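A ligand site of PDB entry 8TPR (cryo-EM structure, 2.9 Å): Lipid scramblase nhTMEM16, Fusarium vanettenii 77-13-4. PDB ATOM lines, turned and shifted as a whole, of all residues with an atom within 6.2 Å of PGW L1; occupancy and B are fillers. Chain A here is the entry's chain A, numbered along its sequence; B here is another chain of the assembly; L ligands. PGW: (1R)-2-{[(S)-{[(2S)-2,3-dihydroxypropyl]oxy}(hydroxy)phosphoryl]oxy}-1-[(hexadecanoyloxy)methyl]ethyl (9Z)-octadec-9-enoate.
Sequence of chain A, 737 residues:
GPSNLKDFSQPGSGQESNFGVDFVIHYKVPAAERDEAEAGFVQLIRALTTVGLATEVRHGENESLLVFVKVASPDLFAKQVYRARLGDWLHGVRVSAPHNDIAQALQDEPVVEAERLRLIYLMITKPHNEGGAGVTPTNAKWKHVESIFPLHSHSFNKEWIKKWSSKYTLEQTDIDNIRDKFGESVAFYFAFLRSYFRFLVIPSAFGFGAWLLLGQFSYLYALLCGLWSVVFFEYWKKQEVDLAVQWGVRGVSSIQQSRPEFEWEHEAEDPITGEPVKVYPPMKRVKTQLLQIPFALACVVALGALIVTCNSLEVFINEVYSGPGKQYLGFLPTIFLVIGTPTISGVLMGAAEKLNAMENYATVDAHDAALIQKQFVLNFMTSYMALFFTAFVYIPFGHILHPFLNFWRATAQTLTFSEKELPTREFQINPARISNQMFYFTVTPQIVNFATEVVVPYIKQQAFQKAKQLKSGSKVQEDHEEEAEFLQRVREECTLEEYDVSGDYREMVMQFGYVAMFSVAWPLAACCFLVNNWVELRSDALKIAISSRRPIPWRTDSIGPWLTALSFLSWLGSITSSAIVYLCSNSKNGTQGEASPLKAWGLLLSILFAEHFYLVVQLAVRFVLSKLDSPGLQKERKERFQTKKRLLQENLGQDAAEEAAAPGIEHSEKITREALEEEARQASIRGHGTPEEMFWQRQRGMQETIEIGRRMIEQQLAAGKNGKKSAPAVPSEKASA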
ATOM      1  N   PHE A 233       1.073   2.874  30.403  1.00  0.00           N
ATOM      2  CA  PHE A 233      -0.269   2.872  29.842  1.00  0.00           C
ATOM      3  C   PHE A 233      -0.985   1.561  30.114  1.00  0.00           C
ATOM      4  O   PHE A 233      -2.145   1.552  30.552  1.00  0.00           O
ATOM      5  CB  PHE A 233      -0.195   3.150  28.335  1.00  0.00           C
ATOM      6  CG  PHE A 233      -1.520   3.134  27.649  1.00  0.00           C
ATOM      7  CD1 PHE A 233      -2.485   4.067  27.966  1.00  0.00           C
ATOM      8  CD2 PHE A 233      -1.808   2.182  26.687  1.00  0.00           C
ATOM      9  CE1 PHE A 233      -3.717   4.054  27.335  1.00  0.00           C
ATOM     10  CE2 PHE A 233      -3.027   2.164  26.052  1.00  0.00           C
ATOM     11  CZ  PHE A 233      -3.983   3.094  26.380  1.00  0.00           C
ATOM     12  N   THR A 564      -7.475   6.898  25.114  1.00  0.00           N
ATOM     13  CA  THR A 564      -7.083   6.899  23.715  1.00  0.00           C
ATOM     14  C   THR A 564      -5.986   7.920  23.453  1.00  0.00           C
ATOM     15  O   THR A 564      -4.950   7.602  22.857  1.00  0.00           O
ATOM     16  CB  THR A 564      -8.297   7.188  22.822  1.00  0.00           C
ATOM     17  OG1 THR A 564      -9.273   6.157  22.993  1.00  0.00           O
ATOM     18  CG2 THR A 564      -7.890   7.244  21.369  1.00  0.00           C
ATOM     19  N   ALA A 565      -6.168   9.132  23.970  1.00  0.00           N
ATOM     20  CA  ALA A 565      -5.163  10.171  23.806  1.00  0.00           C
ATOM     21  C   ALA A 565      -3.800   9.676  24.270  1.00  0.00           C
ATOM     22  O   ALA A 565      -2.808   9.766  23.531  1.00  0.00           O
ATOM     23  CB  ALA A 565      -5.567  11.427  24.581  1.00  0.00           C
ATOM     24  N   SER A 567      -2.640   6.669  24.461  1.00  0.00           N
ATOM     25  CA  SER A 567      -2.106   5.713  23.501  1.00  0.00           C
ATOM     26  C   SER A 567      -1.525   6.454  22.300  1.00  0.00           C
ATOM     27  O   SER A 567      -0.389   6.182  21.883  1.00  0.00           O
ATOM     28  CB  SER A 567      -3.198   4.738  23.056  1.00  0.00           C
ATOM     29  OG  SER A 567      -4.279   5.427  22.462  1.00  0.00           O
ATOM     30  N   PHE A 568      -2.266   7.424  21.774  1.00  0.00           N
ATOM     31  CA  PHE A 568      -1.742   8.219  20.670  1.00  0.00           C
ATOM     32  C   PHE A 568      -0.429   8.875  21.053  1.00  0.00           C
ATOM     33  O   PHE A 568       0.583   8.713  20.373  1.00  0.00           O
ATOM     34  CB  PHE A 568      -2.774   9.262  20.238  1.00  0.00           C
ATOM     35  CG  PHE A 568      -2.300  10.163  19.144  1.00  0.00           C
ATOM     36  CD1 PHE A 568      -2.189   9.703  17.849  1.00  0.00           C
ATOM     37  CD2 PHE A 568      -1.962  11.478  19.410  1.00  0.00           C
ATOM     38  CE1 PHE A 568      -1.756  10.528  16.833  1.00  0.00           C
ATOM     39  CE2 PHE A 568      -1.525  12.307  18.402  1.00  0.00           C
ATOM     40  CZ  PHE A 568      -1.428  11.828  17.113  1.00  0.00           C
ATOM     41  N   TRP A 571       2.281   6.336  20.866  1.00  0.00           N
ATOM     42  CA  TRP A 571       2.691   5.882  19.551  1.00  0.00           C
ATOM     43  C   TRP A 571       3.492   6.950  18.830  1.00  0.00           C
ATOM     44  O   TRP A 571       4.618   6.712  18.383  1.00  0.00           O
ATOM     45  CB  TRP A 571       1.455   5.479  18.744  1.00  0.00           C
ATOM     46  CG  TRP A 571       1.703   5.353  17.276  1.00  0.00           C
ATOM     47  CD1 TRP A 571       2.212   4.275  16.619  1.00  0.00           C
ATOM     48  CD2 TRP A 571       1.430   6.349  16.279  1.00  0.00           C
ATOM     49  NE1 TRP A 571       2.282   4.539  15.275  1.00  0.00           N
ATOM     50  CE2 TRP A 571       1.807   5.797  15.040  1.00  0.00           C
ATOM     51  CE3 TRP A 571       0.909   7.636  16.315  1.00  0.00           C
ATOM     52  CZ2 TRP A 571       1.679   6.508  13.845  1.00  0.00           C
ATOM     53  CZ3 TRP A 571       0.779   8.335  15.128  1.00  0.00           C
ATOM     54  CH2 TRP A 571       1.167   7.773  13.916  1.00  0.00           C
ATOM     55  N   GLU A 611       9.311   2.502  15.873  1.00  0.00           N
ATOM     56  CA  GLU A 611       7.877   2.212  15.855  1.00  0.00           C
ATOM     57  C   GLU A 611       7.606   0.720  16.036  1.00  0.00           C
ATOM     58  O   GLU A 611       6.712   0.328  16.788  1.00  0.00           O
ATOM     59  CB  GLU A 611       7.256   2.729  14.561  1.00  0.00           C
ATOM     60  CG  GLU A 611       5.746   2.837  14.598  1.00  0.00           C
ATOM     61  CD  GLU A 611       5.124   2.632  13.244  1.00  0.00           C
ATOM     62  OE1 GLU A 611       5.867   2.331  12.283  1.00  0.00           O
ATOM     63  OE2 GLU A 611       3.884   2.773  13.131  1.00  0.00           O
ATOM     64  N   TYR A 614       8.249  -0.295  19.528  1.00  0.00           N
ATOM     65  CA  TYR A 614       7.113   0.101  20.352  1.00  0.00           C
ATOM     66  C   TYR A 614       5.975  -0.894  20.222  1.00  0.00           C
ATOM     67  O   TYR A 614       5.373  -1.292  21.219  1.00  0.00           O
ATOM     68  CB  TYR A 614       6.661   1.508  19.949  1.00  0.00           C
ATOM     69  CG  TYR A 614       5.276   1.899  20.438  1.00  0.00           C
ATOM     70  CD1 TYR A 614       5.109   2.489  21.679  1.00  0.00           C
ATOM     71  CD2 TYR A 614       4.157   1.698  19.639  1.00  0.00           C
ATOM     72  CE1 TYR A 614       3.856   2.843  22.128  1.00  0.00           C
ATOM     73  CE2 TYR A 614       2.904   2.051  20.088  1.00  0.00           C
ATOM     74  CZ  TYR A 614       2.755   2.629  21.328  1.00  0.00           C
ATOM     75  OH  TYR A 614       1.509   2.986  21.771  1.00  0.00           O
ATOM     76  N   LEU A 615       5.664  -1.324  18.997  1.00  0.00           N
ATOM     77  CA  LEU A 615       4.580  -2.279  18.804  1.00  0.00           C
ATOM     78  C   LEU A 615       4.894  -3.630  19.442  1.00  0.00           C
ATOM     79  O   LEU A 615       4.025  -4.236  20.087  1.00  0.00           O
ATOM     80  CB  LEU A 615       4.294  -2.452  17.318  1.00  0.00           C
ATOM     81  CG  LEU A 615       3.824  -1.198  16.574  1.00  0.00           C
ATOM     82  CD1 LEU A 615       3.530  -1.515  15.119  1.00  0.00           C
ATOM     83  CD2 LEU A 615       2.604  -0.594  17.246  1.00  0.00           C
ATOM     84  N   GLN A 618       4.608  -3.308  23.123  1.00  0.00           N
ATOM     85  CA  GLN A 618       3.196  -3.248  23.475  1.00  0.00           C
ATOM     86  C   GLN A 618       2.589  -4.642  23.528  1.00  0.00           C
ATOM     87  O   GLN A 618       1.889  -4.991  24.491  1.00  0.00           O
ATOM     88  CB  GLN A 618       2.448  -2.370  22.462  1.00  0.00           C
ATOM     89  CG  GLN A 618       1.343  -1.540  23.064  1.00  0.00           C
ATOM     90  CD  GLN A 618       0.527  -0.816  22.015  1.00  0.00           C
ATOM     91  OE1 GLN A 618       0.556  -1.181  20.841  1.00  0.00           O
ATOM     92  NE2 GLN A 618      -0.206   0.199  22.425  1.00  0.00           N
ATOM     93  N   ARG A 622       1.278  -6.407  26.978  1.00  0.00           N
ATOM     94  CA  ARG A 622      -0.100  -6.871  27.041  1.00  0.00           C
ATOM     95  C   ARG A 622      -0.168  -8.349  27.396  1.00  0.00           C
ATOM     96  O   ARG A 622      -0.968  -8.762  28.243  1.00  0.00           O
ATOM     97  CB  ARG A 622      -0.809  -6.605  25.716  1.00  0.00           C
ATOM     98  CG  ARG A 622      -1.498  -5.264  25.647  1.00  0.00           C
ATOM     99  CD  ARG A 622      -1.909  -4.945  24.221  1.00  0.00           C
ATOM    100  NE  ARG A 622      -2.312  -3.552  24.071  1.00  0.00           N
ATOM    101  CZ  ARG A 622      -2.431  -2.924  22.910  1.00  0.00           C
ATOM    102  NH1 ARG A 622      -2.200  -3.555  21.766  1.00  0.00           N
ATOM    103  NH2 ARG A 622      -2.800  -1.653  22.895  1.00  0.00           N
ATOM    104  N   HIS B 612       1.464   2.317   7.467  1.00  0.00           N
ATOM    105  CA  HIS B 612       0.625   3.284   8.149  1.00  0.00           C
ATOM    106  C   HIS B 612      -0.726   3.438   7.471  1.00  0.00           C
ATOM    107  O   HIS B 612      -1.725   3.694   8.150  1.00  0.00           O
ATOM    108  CB  HIS B 612       1.345   4.626   8.252  1.00  0.00           C
ATOM    109  CG  HIS B 612       2.391   4.649   9.311  1.00  0.00           C
ATOM    110  ND1 HIS B 612       3.512   3.841   9.273  1.00  0.00           N
ATOM    111  CD2 HIS B 612       2.488   5.361  10.463  1.00  0.00           C
ATOM    112  CE1 HIS B 612       4.255   4.076  10.346  1.00  0.00           C
ATOM    113  NE2 HIS B 612       3.653   4.980  11.080  1.00  0.00           N
ATOM    114  N   LEU B 615      -2.657   0.605   8.920  1.00  0.00           N
ATOM    115  CA  LEU B 615      -3.110   0.897  10.280  1.00  0.00           C
ATOM    116  C   LEU B 615      -4.281   1.883  10.283  1.00  0.00           C
ATOM    117  O   LEU B 615      -5.253   1.705  11.016  1.00  0.00           O
ATOM    118  CB  LEU B 615      -1.955   1.430  11.122  1.00  0.00           C
ATOM    119  CG  LEU B 615      -0.776   0.475  11.325  1.00  0.00           C
ATOM    120  CD1 LEU B 615       0.270   1.099  12.214  1.00  0.00           C
ATOM    121  CD2 LEU B 615      -1.256  -0.845  11.908  1.00  0.00           C
ATOM    122  N   VAL B 616      -4.195   2.934   9.460  1.00  0.00           N
ATOM    123  CA  VAL B 616      -5.267   3.925   9.386  1.00  0.00           C
ATOM    124  C   VAL B 616      -6.544   3.295   8.855  1.00  0.00           C
ATOM    125  O   VAL B 616      -7.641   3.548   9.367  1.00  0.00           O
ATOM    126  CB  VAL B 616      -4.820   5.129   8.535  1.00  0.00           C
ATOM    127  CG1 VAL B 616      -5.961   6.113   8.347  1.00  0.00           C
ATOM    128  CG2 VAL B 616      -3.627   5.811   9.177  1.00  0.00           C
ATOM    129  N   LEU B 619      -8.113   1.231  11.597  1.00  0.00           N
ATOM    130  CA  LEU B 619      -8.853   2.061  12.545  1.00  0.00           C
ATOM    131  C   LEU B 619     -10.180   2.529  11.954  1.00  0.00           C
ATOM    132  O   LEU B 619     -11.220   2.498  12.628  1.00  0.00           O
ATOM    133  CB  LEU B 619      -8.009   3.252  12.975  1.00  0.00           C
ATOM    134  CG  LEU B 619      -6.818   2.953  13.885  1.00  0.00           C
ATOM    135  CD1 LEU B 619      -6.055   4.221  14.216  1.00  0.00           C
ATOM    136  CD2 LEU B 619      -7.274   2.252  15.152  1.00  0.00           C
ATOM    137  N   ARG B 622     -12.655  -0.404  11.702  1.00  0.00           N
ATOM    138  CA  ARG B 622     -13.153  -0.742  13.032  1.00  0.00           C
ATOM    139  C   ARG B 622     -14.180   0.273  13.507  1.00  0.00           C
ATOM    140  O   ARG B 622     -15.229  -0.102  14.043  1.00  0.00           O
ATOM    141  CB  ARG B 622     -11.984  -0.822  14.019  1.00  0.00           C
ATOM    142  CG  ARG B 622     -11.375  -2.201  14.137  1.00  0.00           C
ATOM    143  CD  ARG B 622     -10.060  -2.148  14.883  1.00  0.00           C
ATOM    144  NE  ARG B 622      -9.305  -3.394  14.759  1.00  0.00           N
ATOM    145  CZ  ARG B 622      -8.026  -3.528  15.052  1.00  0.00           C
ATOM    146  NH1 ARG B 622      -7.304  -2.501  15.491  1.00  0.00           N
ATOM    147  NH2 ARG B 622      -7.446  -4.709  14.909  1.00  0.00           N
HETATM  148  P   PGW L   1      -5.476   1.583  19.678  1.00  0.00           P
HETATM  149  C01 PGW L   1      -2.093   4.656  17.519  1.00  0.00           C
HETATM  150  C1  PGW L   1      -5.375   5.936  18.447  1.00  0.00           C
HETATM  151  O01 PGW L   1      -4.373   5.399  17.611  1.00  0.00           O
HETATM  152  C02 PGW L   1      -3.421   4.586  18.280  1.00  0.00           C
HETATM  153  C2  PGW L   1      -6.466   6.851  17.845  1.00  0.00           C
HETATM  154  O02 PGW L   1      -5.397   5.682  19.597  1.00  0.00           O
HETATM  155  C03 PGW L   1      -3.904   3.159  18.320  1.00  0.00           C
HETATM  156  C3  PGW L   1      -5.780   8.023  17.102  1.00  0.00           C
HETATM  157  O03 PGW L   1      -2.330   4.966  16.180  1.00  0.00           O
HETATM  158  C4  PGW L   1      -6.053   7.901  15.591  1.00  0.00           C
HETATM  159  O04 PGW L   1      -1.448   2.970  15.711  1.00  0.00           O
HETATM  160  C5  PGW L   1      -5.074   8.791  14.832  1.00  0.00           C
HETATM  161  C6  PGW L   1      -5.557   8.970  13.388  1.00  0.00           C
HETATM  162  C7  PGW L   1      -4.590   9.889  12.629  1.00  0.00           C
HETATM  163  O11 PGW L   1      -4.604   2.961  19.494  1.00  0.00           O
HETATM  164  O12 PGW L   1      -6.862   1.924  20.454  1.00  0.00           O
HETATM  165  O13 PGW L   1      -5.790   1.009  18.315  1.00  0.00           O
HETATM  166  O14 PGW L   1      -4.679   0.584  20.475  1.00  0.00           O
HETATM  167  C19 PGW L   1      -1.842   4.004  15.296  1.00  0.00           C
HETATM  168  C20 PGW L   1      -1.812   4.267  13.794  1.00  0.00           C
HETATM  169  C21 PGW L   1      -1.904   5.757  13.496  1.00  0.00           C
HETATM  170  C22 PGW L   1      -1.525   5.990  12.036  1.00  0.00           C
HETATM  171  C23 PGW L   1      -1.598   7.478  11.692  1.00  0.00           C
HETATM  172  C24 PGW L   1      -0.470   7.834  10.722  1.00  0.00           C
HETATM  173  C25 PGW L   1      -1.007   8.760   9.615  1.00  0.00           C
HETATM  174  P   PGW L   2     -13.321   6.961  22.309  1.00  0.00           P
HETATM  175  C01 PGW L   2     -11.290   9.067  19.521  1.00  0.00           C
HETATM  176  C1  PGW L   2      -9.926  11.393  21.946  1.00  0.00           C
HETATM  177  O01 PGW L   2     -10.829  10.961  20.933  1.00  0.00           O
HETATM  178  C02 PGW L   2     -11.109   9.574  20.951  1.00  0.00           C
HETATM  179  C2  PGW L   2      -8.486  11.835  21.599  1.00  0.00           C
HETATM  180  O02 PGW L   2     -10.282  11.418  23.070  1.00  0.00           O
HETATM  181  C03 PGW L   2     -12.377   9.316  21.737  1.00  0.00           C
HETATM  182  C3  PGW L   2      -8.168  11.529  20.121  1.00  0.00           C
HETATM  183  O03 PGW L   2     -10.511   9.814  18.641  1.00  0.00           O
HETATM  184  C4  PGW L   2      -6.660  11.295  19.959  1.00  0.00           C
HETATM  185  O04 PGW L   2     -12.282   9.902  17.277  1.00  0.00           O
HETATM  186  C5  PGW L   2      -6.272  11.457  18.487  1.00  0.00           C
HETATM  187  C06 PGW L   2      -3.176  17.195  15.329  1.00  0.00           C
HETATM  188  C6  PGW L   2      -6.533  12.902  18.044  1.00  0.00           C
HETATM  189  C7  PGW L   2      -5.785  13.191  16.740  1.00  0.00           C
HETATM  190  C8  PGW L   2      -4.465  13.930  17.055  1.00  0.00           C
HETATM  191  C9  PGW L   2      -4.378  15.214  16.227  1.00  0.00           C
HETATM  192  C10 PGW L   2      -3.253  15.908  16.168  1.00  0.00           C
HETATM  193  O11 PGW L   2     -12.973   8.161  21.253  1.00  0.00           O
HETATM  194  O12 PGW L   2     -14.903   7.054  22.735  1.00  0.00           O
HETATM  195  O13 PGW L   2     -12.458   7.086  23.533  1.00  0.00           O
HETATM  196  O14 PGW L   2     -13.063   5.632  21.650  1.00  0.00           O
HETATM  197  C19 PGW L   2     -11.107  10.001  17.387  1.00  0.00           C
HETATM  198  C20 PGW L   2     -10.252  10.350  16.171  1.00  0.00           C
HETATM  199  C21 PGW L   2     -11.013  11.334  15.290  1.00  0.00           C
HETATM  200  C22 PGW L   2     -10.082  11.903  14.231  1.00  0.00           C
HETATM  201  C23 PGW L   2      -8.891  12.605  14.900  1.00  0.00           C
HETATM  202  C24 PGW L   2      -8.629  13.943  14.195  1.00  0.00           C
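OG of Ser 567 is in hydrogen-bond range of O02 of PGW L1 (3.1 Å).
NH2 of Arg 622 of chain A lies within salt-bridge range of O14 of PGW L1 (3.8 Å).
An oxygen (O13) of PGW L2 is in hydrogen-bond range of the side-chain hydroxyl (OG1) of Thr 564, at 3.4 Å.
CG2 of Thr 564 touches O02 of PGW L1, at 3.4 Å.
Trp 571 touches PGW L1.
CD2 of His 612 of chain B touches C24 of PGW L1, at 3.9 Å.
CB of Leu 615 of chain B touches C20 of PGW L1, 3.9 Å away.
Val 616 of chain B touches PGW L1 (CG2 to C22, 3.6 Å).
Leu 619 of chain B touches PGW L1 (CD2 to O13, 3.7 Å).
Hydrophobic or aromatic side chains within 4 Å of PGW L1: Trp 571, His 612 of chain B, Leu 615 of chain B, Val 616 of chain B and Leu 619 of chain B.
Eight residues have an atom within 4 Å of PGW L1: Thr 564, Ser 567, Trp 571, Arg 622 of chain A, His 612 of chain B, Leu 615 of chain B, Val 616 of chain B and Leu 619 of chain B.
The nearest printed residue that does not touch PGW L1 is Phe 568 (4.03 Å).
The side-chain carboxylate (OE2) of Glu 611 lies within hydrogen-bond range of the indole nitrogen (NE1) of Trp 571 (3.2 Å).
NH2 of Arg 622 of chain A lies close to NE2 of Gln 618 (3.2 Å).
A ring nitrogen (NE2) of His 612 of chain B lies within hydrogen-bond range of the side-chain carboxylate (OE2) of Glu 611.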
